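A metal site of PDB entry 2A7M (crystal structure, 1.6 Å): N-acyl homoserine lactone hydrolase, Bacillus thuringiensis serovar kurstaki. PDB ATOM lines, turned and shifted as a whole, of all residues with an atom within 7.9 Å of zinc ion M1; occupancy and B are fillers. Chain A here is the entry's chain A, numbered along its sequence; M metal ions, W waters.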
ATOM      1  N   CYS A  14      31.705  20.850  23.315  1.00  0.00           N
ATOM      2  CA  CYS A  14      32.126  20.446  24.647  1.00  0.00           C
ATOM      3  C   CYS A  14      32.546  18.992  24.629  1.00  0.00           C
ATOM      4  O   CYS A  14      31.838  18.139  24.106  1.00  0.00           O
ATOM      5  CB  CYS A  14      30.957  20.642  25.625  1.00  0.00           C
ATOM      6  SG  CYS A  14      31.398  20.361  27.341  1.00  0.00           S
ATOM      7  N   LEU A  16      32.991  15.556  26.418  1.00  0.00           N
ATOM      8  CA  LEU A  16      32.509  14.740  27.529  1.00  0.00           C
ATOM      9  C   LEU A  16      33.064  13.351  27.314  1.00  0.00           C
ATOM     10  O   LEU A  16      33.353  12.977  26.181  1.00  0.00           O
ATOM     11  CB  LEU A  16      30.979  14.686  27.562  1.00  0.00           C
ATOM     12  CG  LEU A  16      30.227  15.890  28.135  1.00  0.00           C
ATOM     13  CD1 LEU A  16      30.018  16.957  27.082  1.00  0.00           C
ATOM     14  CD2 LEU A  16      28.888  15.445  28.680  1.00  0.00           C
ATOM     15  N   LEU A  33      31.479  16.972  21.448  1.00  0.00           N
ATOM     16  CA  LEU A  33      30.047  17.046  21.212  1.00  0.00           C
ATOM     17  C   LEU A  33      29.592  18.456  20.847  1.00  0.00           C
ATOM     18  O   LEU A  33      30.113  19.430  21.388  1.00  0.00           O
ATOM     19  CB  LEU A  33      29.290  16.587  22.470  1.00  0.00           C
ATOM     20  CG  LEU A  33      29.433  15.136  22.929  1.00  0.00           C
ATOM     21  CD1 LEU A  33      28.765  14.974  24.273  1.00  0.00           C
ATOM     22  CD2 LEU A  33      28.830  14.176  21.940  1.00  0.00           C
ATOM     23  N   PRO A  34      28.589  18.563  19.967  1.00  0.00           N
ATOM     24  CA  PRO A  34      28.078  19.878  19.571  1.00  0.00           C
ATOM     25  C   PRO A  34      27.281  20.536  20.706  1.00  0.00           C
ATOM     26  O   PRO A  34      26.563  19.857  21.437  1.00  0.00           O
ATOM     27  CB  PRO A  34      27.131  19.553  18.413  1.00  0.00           C
ATOM     28  CG  PRO A  34      26.678  18.152  18.680  1.00  0.00           C
ATOM     29  CD  PRO A  34      27.847  17.460  19.317  1.00  0.00           C
ATOM     30  N   VAL A  35      27.452  21.842  20.853  1.00  0.00           N
ATOM     31  CA  VAL A  35      26.556  22.641  21.687  1.00  0.00           C
ATOM     32  C   VAL A  35      25.674  23.468  20.742  1.00  0.00           C
ATOM     33  O   VAL A  35      26.172  24.062  19.778  1.00  0.00           O
ATOM     34  CB  VAL A  35      27.366  23.540  22.657  1.00  0.00           C
ATOM     35  CG1 VAL A  35      26.442  24.555  23.384  1.00  0.00           C
ATOM     36  CG2 VAL A  35      28.146  22.663  23.676  1.00  0.00           C
ATOM     37  N   TRP A  36      24.374  23.464  20.998  1.00  0.00           N
ATOM     38  CA  TRP A  36      23.406  24.141  20.133  1.00  0.00           C
ATOM     39  C   TRP A  36      22.661  25.250  20.843  1.00  0.00           C
ATOM     40  O   TRP A  36      22.332  25.165  22.039  1.00  0.00           O
ATOM     41  CB  TRP A  36      22.305  23.169  19.695  1.00  0.00           C
ATOM     42  CG  TRP A  36      22.778  22.027  18.887  1.00  0.00           C
ATOM     43  CD1 TRP A  36      22.948  20.756  19.321  1.00  0.00           C
ATOM     44  CD2 TRP A  36      23.108  22.034  17.500  1.00  0.00           C
ATOM     45  NE1 TRP A  36      23.378  19.956  18.302  1.00  0.00           N
ATOM     46  CE2 TRP A  36      23.492  20.715  17.162  1.00  0.00           C
ATOM     47  CE3 TRP A  36      23.127  23.020  16.510  1.00  0.00           C
ATOM     48  CZ2 TRP A  36      23.889  20.354  15.871  1.00  0.00           C
ATOM     49  CZ3 TRP A  36      23.530  22.666  15.228  1.00  0.00           C
ATOM     50  CH2 TRP A  36      23.892  21.343  14.918  1.00  0.00           C
ATOM     51  N   ASP A  50      18.039  28.406  24.430  1.00  0.00           N
ATOM     52  CA  ASP A  50      19.359  28.219  25.035  1.00  0.00           C
ATOM     53  C   ASP A  50      20.380  29.271  24.614  1.00  0.00           C
ATOM     54  O   ASP A  50      20.190  29.974  23.615  1.00  0.00           O
ATOM     55  CB  ASP A  50      19.851  26.755  24.898  1.00  0.00           C
ATOM     56  CG  ASP A  50      19.013  25.775  25.725  1.00  0.00           C
ATOM     57  OD1 ASP A  50      18.269  26.224  26.625  1.00  0.00           O
ATOM     58  OD2 ASP A  50      19.091  24.556  25.450  1.00  0.00           O
ATOM     59  N   SER A 103      16.012  25.340  28.069  1.00  0.00           N
ATOM     60  CA  SER A 103      15.652  23.918  28.182  1.00  0.00           C
ATOM     61  C   SER A 103      15.980  23.395  29.585  1.00  0.00           C
ATOM     62  O   SER A 103      15.207  22.645  30.175  1.00  0.00           O
ATOM     63  CB  SER A 103      16.388  23.088  27.157  1.00  0.00           C
ATOM     64  OG  SER A 103      17.776  23.214  27.340  1.00  0.00           O
ATOM     65  N   HIS A 104      17.148  23.799  30.080  1.00  0.00           N
ATOM     66  CA  HIS A 104      17.574  23.531  31.435  1.00  0.00           C
ATOM     67  C   HIS A 104      18.753  24.448  31.754  1.00  0.00           C
ATOM     68  O   HIS A 104      19.159  25.251  30.881  1.00  0.00           O
ATOM     69  CB  HIS A 104      17.859  22.027  31.662  1.00  0.00           C
ATOM     70  CG  HIS A 104      18.945  21.432  30.820  1.00  0.00           C
ATOM     71  ND1 HIS A 104      19.007  21.521  29.445  1.00  0.00           N
ATOM     72  CD2 HIS A 104      19.973  20.629  31.183  1.00  0.00           C
ATOM     73  CE1 HIS A 104      20.034  20.819  29.002  1.00  0.00           C
ATOM     74  NE2 HIS A 104      20.655  20.278  30.039  1.00  0.00           N
ATOM     75  N   HIS A 106      21.945  23.637  32.838  1.00  0.00           N
ATOM     76  CA  HIS A 106      23.301  23.159  32.691  1.00  0.00           C
ATOM     77  C   HIS A 106      24.132  24.200  31.943  1.00  0.00           C
ATOM     78  O   HIS A 106      23.602  25.003  31.177  1.00  0.00           O
ATOM     79  CB  HIS A 106      23.341  21.834  31.932  1.00  0.00           C
ATOM     80  CG  HIS A 106      22.876  20.667  32.750  1.00  0.00           C
ATOM     81  ND1 HIS A 106      22.660  19.409  32.186  1.00  0.00           N
ATOM     82  CD2 HIS A 106      22.592  20.541  34.068  1.00  0.00           C
ATOM     83  CE1 HIS A 106      22.239  18.586  33.133  1.00  0.00           C
ATOM     84  NE2 HIS A 106      22.195  19.243  34.282  1.00  0.00           N
ATOM     85  N   PHE A 107      25.430  24.167  32.186  1.00  0.00           N
ATOM     86  CA  PHE A 107      26.336  25.233  31.728  1.00  0.00           C
ATOM     87  C   PHE A 107      26.413  25.402  30.202  1.00  0.00           C
ATOM     88  O   PHE A 107      26.719  26.494  29.704  1.00  0.00           O
ATOM     89  CB  PHE A 107      27.738  25.031  32.322  1.00  0.00           C
ATOM     90  CG  PHE A 107      28.705  24.312  31.411  1.00  0.00           C
ATOM     91  CD1 PHE A 107      29.762  25.010  30.827  1.00  0.00           C
ATOM     92  CD2 PHE A 107      28.543  22.969  31.107  1.00  0.00           C
ATOM     93  CE1 PHE A 107      30.657  24.363  29.969  1.00  0.00           C
ATOM     94  CE2 PHE A 107      29.431  22.314  30.240  1.00  0.00           C
ATOM     95  CZ  PHE A 107      30.471  23.019  29.671  1.00  0.00           C
ATOM     96  N   ASP A 108      26.143  24.312  29.476  1.00  0.00           N
ATOM     97  CA  ASP A 108      26.153  24.359  28.006  1.00  0.00           C
ATOM     98  C   ASP A 108      24.829  24.846  27.416  1.00  0.00           C
ATOM     99  O   ASP A 108      24.711  24.940  26.202  1.00  0.00           O
ATOM    100  CB  ASP A 108      26.586  23.005  27.404  1.00  0.00           C
ATOM    101  CG  ASP A 108      25.770  21.814  27.907  1.00  0.00           C
ATOM    102  OD1 ASP A 108      25.373  20.985  27.065  1.00  0.00           O
ATOM    103  OD2 ASP A 108      25.528  21.685  29.141  1.00  0.00           O
ATOM    104  N   HIS A 109      23.860  25.203  28.282  1.00  0.00           N
ATOM    105  CA  HIS A 109      22.535  25.660  27.855  1.00  0.00           C
ATOM    106  C   HIS A 109      22.138  27.018  28.400  1.00  0.00           C
ATOM    107  O   HIS A 109      21.309  27.700  27.791  1.00  0.00           O
ATOM    108  CB  HIS A 109      21.498  24.612  28.282  1.00  0.00           C
ATOM    109  CG  HIS A 109      21.748  23.287  27.638  1.00  0.00           C
ATOM    110  ND1 HIS A 109      21.130  22.917  26.461  1.00  0.00           N
ATOM    111  CD2 HIS A 109      22.622  22.303  27.938  1.00  0.00           C
ATOM    112  CE1 HIS A 109      21.586  21.730  26.087  1.00  0.00           C
ATOM    113  NE2 HIS A 109      22.491  21.331  26.982  1.00  0.00           N
ATOM    114  N   HIS A 169      17.027  14.083  32.844  1.00  0.00           N
ATOM    115  CA  HIS A 169      18.393  14.501  32.561  1.00  0.00           C
ATOM    116  C   HIS A 169      18.814  15.593  33.547  1.00  0.00           C
ATOM    117  O   HIS A 169      19.950  15.628  33.993  1.00  0.00           O
ATOM    118  CB  HIS A 169      18.507  15.026  31.140  1.00  0.00           C
ATOM    119  CG  HIS A 169      19.813  15.700  30.881  1.00  0.00           C
ATOM    120  ND1 HIS A 169      21.013  15.015  30.813  1.00  0.00           N
ATOM    121  CD2 HIS A 169      20.113  17.003  30.647  1.00  0.00           C
ATOM    122  CE1 HIS A 169      21.988  15.868  30.573  1.00  0.00           C
ATOM    123  NE2 HIS A 169      21.466  17.085  30.447  1.00  0.00           N
ATOM    124  N   HIS A 173      14.146  19.626  33.233  1.00  0.00           N
ATOM    125  CA  HIS A 173      14.443  19.686  31.806  1.00  0.00           C
ATOM    126  C   HIS A 173      13.143  19.786  30.984  1.00  0.00           C
ATOM    127  O   HIS A 173      12.136  19.142  31.316  1.00  0.00           O
ATOM    128  CB  HIS A 173      15.266  18.472  31.364  1.00  0.00           C
ATOM    129  CG  HIS A 173      15.521  18.453  29.895  1.00  0.00           C
ATOM    130  ND1 HIS A 173      16.684  18.951  29.324  1.00  0.00           N
ATOM    131  CD2 HIS A 173      14.733  18.076  28.864  1.00  0.00           C
ATOM    132  CE1 HIS A 173      16.596  18.842  28.006  1.00  0.00           C
ATOM    133  NE2 HIS A 173      15.429  18.309  27.707  1.00  0.00           N
ATOM    134  N   ILE A 190      16.144  18.249  22.925  1.00  0.00           N
ATOM    135  CA  ILE A 190      17.263  18.780  23.694  1.00  0.00           C
ATOM    136  C   ILE A 190      17.876  17.630  24.449  1.00  0.00           C
ATOM    137  O   ILE A 190      18.109  16.583  23.854  1.00  0.00           O
ATOM    138  CB  ILE A 190      16.862  19.969  24.611  1.00  0.00           C
ATOM    139  CG1 ILE A 190      15.818  20.878  23.908  1.00  0.00           C
ATOM    140  CG2 ILE A 190      18.117  20.740  25.040  1.00  0.00           C
ATOM    141  CD1 ILE A 190      16.349  21.699  22.722  1.00  0.00           C
ATOM    142  N   ASP A 191      18.130  17.762  25.743  1.00  0.00           N
ATOM    143  CA  ASP A 191      18.881  16.716  26.440  1.00  0.00           C
ATOM    144  C   ASP A 191      18.014  15.594  27.053  1.00  0.00           C
ATOM    145  O   ASP A 191      18.489  14.815  27.885  1.00  0.00           O
ATOM    146  CB  ASP A 191      19.855  17.320  27.467  1.00  0.00           C
ATOM    147  CG  ASP A 191      21.043  18.061  26.805  1.00  0.00           C
ATOM    148  OD1 ASP A 191      21.054  18.217  25.571  1.00  0.00           O
ATOM    149  OD2 ASP A 191      21.970  18.507  27.534  1.00  0.00           O
ATOM    150  N   TYR A 194      20.518  12.614  24.376  1.00  0.00           N
ATOM    151  CA  TYR A 194      21.711  13.128  23.692  1.00  0.00           C
ATOM    152  C   TYR A 194      21.756  12.639  22.245  1.00  0.00           C
ATOM    153  O   TYR A 194      22.027  13.416  21.331  1.00  0.00           O
ATOM    154  CB  TYR A 194      22.990  12.664  24.393  1.00  0.00           C
ATOM    155  CG  TYR A 194      23.394  13.451  25.632  1.00  0.00           C
ATOM    156  CD1 TYR A 194      22.521  14.321  26.277  1.00  0.00           C
ATOM    157  CD2 TYR A 194      24.661  13.277  26.162  1.00  0.00           C
ATOM    158  CE1 TYR A 194      22.918  15.017  27.410  1.00  0.00           C
ATOM    159  CE2 TYR A 194      25.062  13.949  27.290  1.00  0.00           C
ATOM    160  CZ  TYR A 194      24.185  14.810  27.915  1.00  0.00           C
ATOM    161  OH  TYR A 194      24.621  15.464  29.034  1.00  0.00           O
ATOM    162  N   GLY A 234      19.982  16.104  21.357  1.00  0.00           N
ATOM    163  CA  GLY A 234      20.727  17.181  22.034  1.00  0.00           C
ATOM    164  C   GLY A 234      22.197  17.295  21.714  1.00  0.00           C
ATOM    165  O   GLY A 234      22.730  18.396  21.572  1.00  0.00           O
ATOM    166  N   HIS A 235      22.879  16.161  21.613  1.00  0.00           N
ATOM    167  CA  HIS A 235      24.333  16.152  21.537  1.00  0.00           C
ATOM    168  C   HIS A 235      24.749  14.955  20.677  1.00  0.00           C
ATOM    169  O   HIS A 235      25.416  14.018  21.165  1.00  0.00           O
ATOM    170  CB  HIS A 235      24.960  16.051  22.936  1.00  0.00           C
ATOM    171  CG  HIS A 235      24.790  17.272  23.808  1.00  0.00           C
ATOM    172  ND1 HIS A 235      25.390  18.482  23.539  1.00  0.00           N
ATOM    173  CD2 HIS A 235      24.111  17.435  24.973  1.00  0.00           C
ATOM    174  CE1 HIS A 235      25.067  19.347  24.481  1.00  0.00           C
ATOM    175  NE2 HIS A 235      24.296  18.736  25.364  1.00  0.00           N
HETATM  176 ZN    ZN M   1      23.573  19.636  27.128  1.00  0.00          ZN
HETATM  177 ZN    ZN M   2      22.274  18.973  30.120  1.00  0.00          ZN
HETATM  178  O   HOH W   1      23.994  19.296  29.030  1.00  0.00           O
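ND1 of His 235 is in hydrogen-bond range of O of Pro 34 (2.8 Å).
The backbone NH of Asp 191 sits close to a ring nitrogen (NE2) of His 173 (3.4 Å).
ND1 of His 109 sits at hydrogen-bond distance from OG of Ser 103 (3.5 Å).
ND1 of His 109 lies within hydrogen-bond range of OD2 of Asp 50, at 2.8 Å.
The backbone carbonyl oxygen (O) of Tyr 194 lies within hydrogen-bond range of the backbone NH (N) of His 235, at 2.9 Å.
Four residues have an atom within 4 Å of zinc ion M1: Asp 108, His 109, Asp 191 and His 235.
Zinc ion M1 is bound by water W1 (2.0 Å), the side-chain carboxylate of Asp 191 (2.0 Å), a ring nitrogen (NE2) of His 109 (2.0 Å), a ring nitrogen (NE2) of His 235 (2.1 Å) and the side-chain carboxylate of Asp 108 (2.3 Å).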
